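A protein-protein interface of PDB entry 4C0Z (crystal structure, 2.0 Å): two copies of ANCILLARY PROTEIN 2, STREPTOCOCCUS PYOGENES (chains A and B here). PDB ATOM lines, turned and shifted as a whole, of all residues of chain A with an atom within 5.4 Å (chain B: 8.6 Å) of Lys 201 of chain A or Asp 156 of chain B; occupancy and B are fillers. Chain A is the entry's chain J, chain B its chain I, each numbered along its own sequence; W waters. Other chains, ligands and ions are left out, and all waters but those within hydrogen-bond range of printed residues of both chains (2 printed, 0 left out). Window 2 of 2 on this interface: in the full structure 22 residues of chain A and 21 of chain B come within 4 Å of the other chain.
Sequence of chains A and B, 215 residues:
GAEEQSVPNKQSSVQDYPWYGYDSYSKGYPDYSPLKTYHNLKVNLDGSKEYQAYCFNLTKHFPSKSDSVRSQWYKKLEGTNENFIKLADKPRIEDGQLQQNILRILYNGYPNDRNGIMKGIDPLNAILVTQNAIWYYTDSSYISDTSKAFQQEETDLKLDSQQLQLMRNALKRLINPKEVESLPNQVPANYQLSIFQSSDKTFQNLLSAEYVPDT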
ATOM      1  N   LYS A  60      18.900  14.600 -30.692  1.00  0.00           N
ATOM      2  CA  LYS A  60      18.187  15.885 -30.774  1.00  0.00           C
ATOM      3  C   LYS A  60      16.727  15.639 -31.145  1.00  0.00           C
ATOM      4  O   LYS A  60      16.364  14.497 -31.370  1.00  0.00           O
ATOM      5  CB  LYS A  60      18.889  16.871 -31.730  1.00  0.00           C
ATOM      6  CG  LYS A  60      20.193  17.346 -31.124  1.00  0.00           C
ATOM      7  CD  LYS A  60      20.956  18.242 -32.023  1.00  0.00           C
ATOM      8  CE  LYS A  60      22.207  18.743 -31.328  1.00  0.00           C
ATOM      9  NZ  LYS A  60      22.677  20.019 -31.942  1.00  0.00           N
ATOM     10  N   LEU A  87      28.730  19.466 -37.574  1.00  0.00           N
ATOM     11  CA  LEU A  87      27.337  19.357 -37.107  1.00  0.00           C
ATOM     12  C   LEU A  87      26.886  17.985 -36.582  1.00  0.00           C
ATOM     13  O   LEU A  87      25.878  17.907 -35.884  1.00  0.00           O
ATOM     14  CB  LEU A  87      26.385  19.812 -38.235  1.00  0.00           C
ATOM     15  CG  LEU A  87      26.508  21.285 -38.646  1.00  0.00           C
ATOM     16  CD1 LEU A  87      25.717  21.562 -39.905  1.00  0.00           C
ATOM     17  CD2 LEU A  87      26.040  22.209 -37.533  1.00  0.00           C
ATOM     18  N   GLN A 197      21.343  23.069 -41.770  1.00  0.00           N
ATOM     19  CA  GLN A 197      21.705  23.362 -40.394  1.00  0.00           C
ATOM     20  C   GLN A 197      20.530  24.005 -39.675  1.00  0.00           C
ATOM     21  O   GLN A 197      20.056  25.067 -40.086  1.00  0.00           O
ATOM     22  CB  GLN A 197      22.959  24.250 -40.331  1.00  0.00           C
ATOM     23  CG  GLN A 197      23.377  24.603 -38.894  1.00  0.00           C
ATOM     24  CD  GLN A 197      24.552  25.554 -38.818  1.00  0.00           C
ATOM     25  OE1 GLN A 197      25.121  25.963 -39.810  1.00  0.00           O
ATOM     26  NE2 GLN A 197      24.929  25.944 -37.630  1.00  0.00           N
ATOM     27  N   SER A 198      20.099  23.379 -38.586  1.00  0.00           N
ATOM     28  CA  SER A 198      18.990  23.874 -37.789  1.00  0.00           C
ATOM     29  C   SER A 198      19.393  25.160 -37.048  1.00  0.00           C
ATOM     30  O   SER A 198      20.437  25.187 -36.405  1.00  0.00           O
ATOM     31  CB  SER A 198      18.559  22.804 -36.779  1.00  0.00           C
ATOM     32  OG  SER A 198      17.428  23.245 -36.058  1.00  0.00           O
ATOM     33  N   SER A 199      18.533  26.192 -37.097  1.00  0.00           N
ATOM     34  CA  SER A 199      18.729  27.451 -36.350  1.00  0.00           C
ATOM     35  C   SER A 199      18.634  27.163 -34.831  1.00  0.00           C
ATOM     36  O   SER A 199      19.389  27.720 -34.044  1.00  0.00           O
ATOM     37  CB  SER A 199      17.666  28.474 -36.736  1.00  0.00           C
ATOM     38  OG  SER A 199      17.817  29.668 -35.990  1.00  0.00           O
ATOM     39  N   ASP A 200      17.705  26.291 -34.449  1.00  0.00           N
ATOM     40  CA  ASP A 200      17.490  25.873 -33.084  1.00  0.00           C
ATOM     41  C   ASP A 200      18.385  24.616 -32.873  1.00  0.00           C
ATOM     42  O   ASP A 200      18.122  23.575 -33.463  1.00  0.00           O
ATOM     43  CB  ASP A 200      15.983  25.537 -32.902  1.00  0.00           C
ATOM     44  CG  ASP A 200      15.565  25.218 -31.478  1.00  0.00           C
ATOM     45  OD1 ASP A 200      16.443  24.798 -30.670  1.00  0.00           O
ATOM     46  OD2 ASP A 200      14.379  25.427 -31.155  1.00  0.00           O
ATOM     47  N   LYS A 201      19.403  24.715 -32.006  1.00  0.00           N
ATOM     48  CA  LYS A 201      20.362  23.647 -31.711  1.00  0.00           C
ATOM     49  C   LYS A 201      19.752  22.417 -30.989  1.00  0.00           C
ATOM     50  O   LYS A 201      20.383  21.364 -30.897  1.00  0.00           O
ATOM     51  CB  LYS A 201      21.579  24.201 -30.941  1.00  0.00           C
ATOM     52  CG  LYS A 201      22.467  25.154 -31.758  1.00  0.00           C
ATOM     53  CD  LYS A 201      23.257  24.417 -32.820  1.00  0.00           C
ATOM     54  CE  LYS A 201      24.175  25.280 -33.640  1.00  0.00           C
ATOM     55  NZ  LYS A 201      24.774  24.483 -34.756  1.00  0.00           N
ATOM     56  N   THR A 202      18.519  22.533 -30.547  1.00  0.00           N
ATOM     57  CA  THR A 202      17.779  21.469 -29.870  1.00  0.00           C
ATOM     58  C   THR A 202      17.170  20.476 -30.913  1.00  0.00           C
ATOM     59  O   THR A 202      16.758  19.371 -30.570  1.00  0.00           O
ATOM     60  CB  THR A 202      16.812  22.230 -28.968  1.00  0.00           C
ATOM     61  OG1 THR A 202      17.214  22.134 -27.597  1.00  0.00           O
ATOM     62  CG2 THR A 202      15.416  21.913 -29.178  1.00  0.00           C
ATOM     63  N   PHE A 203      17.075  20.907 -32.174  1.00  0.00           N
ATOM     64  CA  PHE A 203      16.487  20.114 -33.258  1.00  0.00           C
ATOM     65  C   PHE A 203      17.524  19.516 -34.171  1.00  0.00           C
ATOM     66  O   PHE A 203      18.613  20.087 -34.363  1.00  0.00           O
ATOM     67  CB  PHE A 203      15.466  20.944 -34.062  1.00  0.00           C
ATOM     68  CG  PHE A 203      14.163  21.127 -33.320  1.00  0.00           C
ATOM     69  CD1 PHE A 203      14.000  22.166 -32.406  1.00  0.00           C
ATOM     70  CD2 PHE A 203      13.102  20.236 -33.505  1.00  0.00           C
ATOM     71  CE1 PHE A 203      12.809  22.283 -31.654  1.00  0.00           C
ATOM     72  CE2 PHE A 203      11.913  20.371 -32.787  1.00  0.00           C
ATOM     73  CZ  PHE A 203      11.763  21.394 -31.874  1.00  0.00           C
ATOM     74  N   SER B  33      16.932  27.185 -20.275  1.00  0.00           N
ATOM     75  CA  SER B  33      17.006  27.817 -21.589  1.00  0.00           C
ATOM     76  C   SER B  33      16.410  26.839 -22.608  1.00  0.00           C
ATOM     77  O   SER B  33      16.847  25.686 -22.659  1.00  0.00           O
ATOM     78  CB  SER B  33      18.442  28.170 -21.965  1.00  0.00           C
ATOM     79  OG  SER B  33      18.429  28.597 -23.312  1.00  0.00           O
ATOM     80  N   PRO B  34      15.442  27.276 -23.445  1.00  0.00           N
ATOM     81  CA  PRO B  34      14.874  26.366 -24.445  1.00  0.00           C
ATOM     82  C   PRO B  34      15.833  26.052 -25.612  1.00  0.00           C
ATOM     83  O   PRO B  34      15.519  25.203 -26.440  1.00  0.00           O
ATOM     84  CB  PRO B  34      13.623  27.104 -24.919  1.00  0.00           C
ATOM     85  CG  PRO B  34      13.930  28.517 -24.730  1.00  0.00           C
ATOM     86  CD  PRO B  34      14.837  28.622 -23.538  1.00  0.00           C
ATOM     87  N   LEU B  35      17.000  26.713 -25.650  1.00  0.00           N
ATOM     88  CA  LEU B  35      18.008  26.520 -26.686  1.00  0.00           C
ATOM     89  C   LEU B  35      19.111  25.544 -26.261  1.00  0.00           C
ATOM     90  O   LEU B  35      19.961  25.207 -27.078  1.00  0.00           O
ATOM     91  CB  LEU B  35      18.620  27.875 -27.109  1.00  0.00           C
ATOM     92  CG  LEU B  35      17.665  28.967 -27.573  1.00  0.00           C
ATOM     93  CD1 LEU B  35      18.452  30.201 -27.950  1.00  0.00           C
ATOM     94  CD2 LEU B  35      16.793  28.501 -28.747  1.00  0.00           C
ATOM     95  N   LYS B  36      19.080  25.076 -25.003  1.00  0.00           N
ATOM     96  CA  LYS B  36      20.071  24.144 -24.461  1.00  0.00           C
ATOM     97  C   LYS B  36      19.576  22.717 -24.560  1.00  0.00           C
ATOM     98  O   LYS B  36      18.417  22.438 -24.241  1.00  0.00           O
ATOM     99  CB  LYS B  36      20.440  24.512 -23.017  1.00  0.00           C
ATOM    100  CG  LYS B  36      21.363  25.717 -22.932  1.00  0.00           C
ATOM    101  CD  LYS B  36      21.797  25.998 -21.506  1.00  0.00           C
ATOM    102  CE  LYS B  36      22.718  27.188 -21.440  1.00  0.00           C
ATOM    103  NZ  LYS B  36      23.176  27.451 -20.050  1.00  0.00           N
ATOM    104  N   THR B  37      20.450  21.816 -25.006  1.00  0.00           N
ATOM    105  CA  THR B  37      20.146  20.390 -25.196  1.00  0.00           C
ATOM    106  C   THR B  37      20.163  19.573 -23.878  1.00  0.00           C
ATOM    107  O   THR B  37      20.429  18.367 -23.909  1.00  0.00           O
ATOM    108  CB  THR B  37      21.106  19.778 -26.242  1.00  0.00           C
ATOM    109  OG1 THR B  37      22.461  20.086 -25.869  1.00  0.00           O
ATOM    110  CG2 THR B  37      20.799  20.238 -27.656  1.00  0.00           C
ATOM    111  N   TYR B  38      19.847  20.205 -22.741  1.00  0.00           N
ATOM    112  CA  TYR B  38      19.804  19.477 -21.482  1.00  0.00           C
ATOM    113  C   TYR B  38      18.447  18.764 -21.345  1.00  0.00           C
ATOM    114  O   TYR B  38      17.473  19.137 -22.000  1.00  0.00           O
ATOM    115  CB  TYR B  38      19.987  20.433 -20.290  1.00  0.00           C
ATOM    116  CG  TYR B  38      21.390  20.938 -20.046  1.00  0.00           C
ATOM    117  CD1 TYR B  38      22.464  20.054 -19.944  1.00  0.00           C
ATOM    118  CD2 TYR B  38      21.629  22.287 -19.774  1.00  0.00           C
ATOM    119  CE1 TYR B  38      23.751  20.509 -19.649  1.00  0.00           C
ATOM    120  CE2 TYR B  38      22.911  22.753 -19.481  1.00  0.00           C
ATOM    121  CZ  TYR B  38      23.970  21.861 -19.413  1.00  0.00           C
ATOM    122  OH  TYR B  38      25.243  22.335 -19.135  1.00  0.00           O
ATOM    123  N   LEU B 128      23.552  14.410 -18.225  1.00  0.00           N
ATOM    124  CA  LEU B 128      23.976  14.239 -19.613  1.00  0.00           C
ATOM    125  C   LEU B 128      25.018  13.094 -19.758  1.00  0.00           C
ATOM    126  O   LEU B 128      24.890  12.282 -20.658  1.00  0.00           O
ATOM    127  CB  LEU B 128      24.518  15.573 -20.151  1.00  0.00           C
ATOM    128  CG  LEU B 128      24.650  15.679 -21.642  1.00  0.00           C
ATOM    129  CD1 LEU B 128      24.181  17.026 -22.123  1.00  0.00           C
ATOM    130  CD2 LEU B 128      26.083  15.472 -22.062  1.00  0.00           C
ATOM    131  N   PHE B 150      31.365  14.609 -26.389  1.00  0.00           N
ATOM    132  CA  PHE B 150      30.664  15.862 -26.093  1.00  0.00           C
ATOM    133  C   PHE B 150      31.138  17.076 -26.925  1.00  0.00           C
ATOM    134  O   PHE B 150      31.020  18.212 -26.462  1.00  0.00           O
ATOM    135  CB  PHE B 150      30.686  16.176 -24.584  1.00  0.00           C
ATOM    136  CG  PHE B 150      30.339  15.006 -23.695  1.00  0.00           C
ATOM    137  CD1 PHE B 150      29.073  14.422 -23.741  1.00  0.00           C
ATOM    138  CD2 PHE B 150      31.276  14.476 -22.822  1.00  0.00           C
ATOM    139  CE1 PHE B 150      28.760  13.322 -22.934  1.00  0.00           C
ATOM    140  CE2 PHE B 150      30.959  13.382 -22.005  1.00  0.00           C
ATOM    141  CZ  PHE B 150      29.698  12.823 -22.054  1.00  0.00           C
ATOM    142  N   GLN B 151      31.609  16.841 -28.172  1.00  0.00           N
ATOM    143  CA  GLN B 151      32.041  17.921 -29.056  1.00  0.00           C
ATOM    144  C   GLN B 151      30.879  18.852 -29.444  1.00  0.00           C
ATOM    145  O   GLN B 151      31.043  20.077 -29.401  1.00  0.00           O
ATOM    146  CB  GLN B 151      32.776  17.378 -30.279  1.00  0.00           C
ATOM    147  CG  GLN B 151      34.276  17.207 -30.033  1.00  0.00           C
ATOM    148  CD  GLN B 151      35.004  16.707 -31.259  1.00  0.00           C
ATOM    149  OE1 GLN B 151      34.975  17.324 -32.337  1.00  0.00           O
ATOM    150  NE2 GLN B 151      35.696  15.588 -31.115  1.00  0.00           N
ATOM    151  N   GLN B 152      29.704  18.282 -29.774  1.00  0.00           N
ATOM    152  CA  GLN B 152      28.507  19.068 -30.117  1.00  0.00           C
ATOM    153  C   GLN B 152      27.969  19.794 -28.883  1.00  0.00           C
ATOM    154  O   GLN B 152      27.650  20.981 -28.968  1.00  0.00           O
ATOM    155  CB  GLN B 152      27.407  18.202 -30.775  1.00  0.00           C
ATOM    156  CG  GLN B 152      27.725  17.734 -32.201  1.00  0.00           C
ATOM    157  CD  GLN B 152      27.947  18.840 -33.212  1.00  0.00           C
ATOM    158  OE1 GLN B 152      27.128  19.747 -33.386  1.00  0.00           O
ATOM    159  NE2 GLN B 152      29.055  18.754 -33.923  1.00  0.00           N
ATOM    160  N   GLU B 153      27.926  19.094 -27.734  1.00  0.00           N
ATOM    161  CA  GLU B 153      27.498  19.637 -26.436  1.00  0.00           C
ATOM    162  C   GLU B 153      28.412  20.790 -25.996  1.00  0.00           C
ATOM    163  O   GLU B 153      27.924  21.758 -25.418  1.00  0.00           O
ATOM    164  CB  GLU B 153      27.480  18.537 -25.361  1.00  0.00           C
ATOM    165  CG  GLU B 153      26.372  17.507 -25.525  1.00  0.00           C
ATOM    166  CD  GLU B 153      26.652  16.308 -26.420  1.00  0.00           C
ATOM    167  OE1 GLU B 153      27.621  16.350 -27.215  1.00  0.00           O
ATOM    168  OE2 GLU B 153      25.877  15.326 -26.339  1.00  0.00           O
ATOM    169  N   GLU B 154      29.727  20.700 -26.300  1.00  0.00           N
ATOM    170  CA  GLU B 154      30.709  21.742 -25.974  1.00  0.00           C
ATOM    171  C   GLU B 154      30.315  23.068 -26.624  1.00  0.00           C
ATOM    172  O   GLU B 154      30.359  24.093 -25.949  1.00  0.00           O
ATOM    173  CB  GLU B 154      32.128  21.338 -26.411  1.00  0.00           C
ATOM    174  CG  GLU B 154      33.217  22.299 -25.946  1.00  0.00           C
ATOM    175  CD  GLU B 154      34.590  22.150 -26.580  1.00  0.00           C
ATOM    176  OE1 GLU B 154      34.824  21.149 -27.300  1.00  0.00           O
ATOM    177  OE2 GLU B 154      35.449  23.026 -26.323  1.00  0.00           O
ATOM    178  N   THR B 155      29.935  23.052 -27.920  1.00  0.00           N
ATOM    179  CA  THR B 155      29.542  24.269 -28.635  1.00  0.00           C
ATOM    180  C   THR B 155      28.096  24.661 -28.325  1.00  0.00           C
ATOM    181  O   THR B 155      27.840  25.851 -28.122  1.00  0.00           O
ATOM    182  CB  THR B 155      29.847  24.196 -30.143  1.00  0.00           C
ATOM    183  OG1 THR B 155      29.294  23.007 -30.698  1.00  0.00           O
ATOM    184  CG2 THR B 155      31.343  24.251 -30.443  1.00  0.00           C
ATOM    185  N   ASP B 156      27.159  23.683 -28.259  1.00  0.00           N
ATOM    186  CA  ASP B 156      25.744  23.956 -27.967  1.00  0.00           C
ATOM    187  C   ASP B 156      25.478  24.473 -26.550  1.00  0.00           C
ATOM    188  O   ASP B 156      24.640  25.358 -26.389  1.00  0.00           O
ATOM    189  CB  ASP B 156      24.861  22.731 -28.253  1.00  0.00           C
ATOM    190  CG  ASP B 156      24.783  22.259 -29.707  1.00  0.00           C
ATOM    191  OD1 ASP B 156      25.291  22.980 -30.604  1.00  0.00           O
ATOM    192  OD2 ASP B 156      24.241  21.162 -29.942  1.00  0.00           O
ATOM    193  N   LEU B 157      26.167  23.911 -25.530  1.00  0.00           N
ATOM    194  CA  LEU B 157      25.989  24.267 -24.113  1.00  0.00           C
ATOM    195  C   LEU B 157      27.078  25.211 -23.603  1.00  0.00           C
ATOM    196  O   LEU B 157      26.985  25.689 -22.466  1.00  0.00           O
ATOM    197  CB  LEU B 157      25.925  22.999 -23.225  1.00  0.00           C
ATOM    198  CG  LEU B 157      24.886  21.922 -23.596  1.00  0.00           C
ATOM    199  CD1 LEU B 157      25.256  20.587 -23.025  1.00  0.00           C
ATOM    200  CD2 LEU B 157      23.499  22.304 -23.152  1.00  0.00           C
ATOM    201  N   LYS B 158      28.105  25.480 -24.444  1.00  0.00           N
ATOM    202  CA  LYS B 158      29.281  26.325 -24.123  1.00  0.00           C
ATOM    203  C   LYS B 158      29.926  25.877 -22.798  1.00  0.00           C
ATOM    204  O   LYS B 158      29.961  26.621 -21.811  1.00  0.00           O
ATOM    205  CB  LYS B 158      28.959  27.834 -24.184  1.00  0.00           C
ATOM    206  CG  LYS B 158      28.467  28.286 -25.563  1.00  0.00           C
ATOM    207  CD  LYS B 158      29.033  29.642 -25.968  1.00  0.00           C
ATOM    208  CE  LYS B 158      28.944  29.894 -27.454  1.00  0.00           C
ATOM    209  NZ  LYS B 158      29.935  29.092 -28.227  1.00  0.00           N
ATOM    210  N   LEU B 159      30.361  24.604 -22.781  1.00  0.00           N
ATOM    211  CA  LEU B 159      30.996  23.965 -21.623  1.00  0.00           C
ATOM    212  C   LEU B 159      32.432  24.443 -21.512  1.00  0.00           C
ATOM    213  O   LEU B 159      33.150  24.466 -22.518  1.00  0.00           O
ATOM    214  CB  LEU B 159      30.993  22.419 -21.761  1.00  0.00           C
ATOM    215  CG  LEU B 159      29.669  21.694 -22.037  1.00  0.00           C
ATOM    216  CD1 LEU B 159      29.916  20.245 -22.428  1.00  0.00           C
ATOM    217  CD2 LEU B 159      28.729  21.774 -20.846  1.00  0.00           C
HETATM  218  O   HOH W   1      13.859  25.408 -28.555  1.00  0.00           O
HETATM  219  O   HOH W   2      24.521  20.051 -34.708  1.00  0.00           O
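The backbone carbonyl oxygen (O) of Leu 87 of chain A lies close to the side-chain amide oxygen (OE1) of Gln 152 of chain B (3.3 Å). NZ of Lys 60 of chain A lies within salt-bridge range of OD2 of Asp 156 of chain B.
The side-chain amino group of Lys 60 of chain A sits at hydrogen-bond distance from the backbone carbonyl oxygen of Lys 201 of chain A, 2.9 Å away. The side-chain amide nitrogen (NE2) of Gln 197 of chain A lies close to the side-chain amino group (NZ) of Lys 201 of chain A (3.2 Å). The backbone carbonyl oxygen of Gln 152 of chain B sits at hydrogen-bond distance from the side-chain hydroxyl of Thr 155 of chain B (3.1 Å). OD1 of Asp 200 of chain A sits at hydrogen-bond distance from N of Thr 202 of chain A, 3.1 Å away.
Among the printed residues, pairs that only touch across the chains: Lys 201 of chain A with Thr 37 of chain B (3.5 Å), Lys 201 of chain A with Asp 156 of chain B (3.3 Å), Thr 202 of chain A with Pro 34 of chain B (3.7 Å), Thr 202 of chain A with Lys 36 of chain B (3.6 Å) and Thr 202 of chain A with Thr 37 of chain B (3.9 Å).
Lys 201 of chain A touches two residues of chain B. Asp 156 of chain B touches two residues of chain A. Of the printed residues of chain B, Leu 87 of chain A touches Gln 152. Printed residues of chain A within 4 Å of Thr 37 of chain B: Lys 201 and Thr 202. The nearest printed residue of chain A that does not touch Asp 156 of chain B is Thr 202 of chain A (5.9 Å). The nearest printed residue of chain A that does not touch Thr 37 of chain B is Lys 60 of chain A (4.2 Å).
Of the 17 printed residues of chain B, 5 touch a printed residue of chain A. Of the 9 printed residues of chain A, 4 touch a printed residue of chain B. Along chain A the printed residues that touch a printed residue of chain B span positions 60 to 202. Among the printed residues, Asp or Glu carboxylates within 4 Å of a Lys or Arg side-chain nitrogen of the other chain: Lys 60 of chain A with Asp 156 of chain B.
No position is printed for both chains.
Water W1 bridges the side-chain carboxylate of Asp 200 of chain A (2.7 Å) and the backbone carbonyl oxygen of Pro 34 of chain B (2.7 Å). Water W2 lies within hydrogen-bond range of O of Leu 87 of chain A, OE1 of Gln 152 of chain B and NZ of Lys 60 of chain A.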
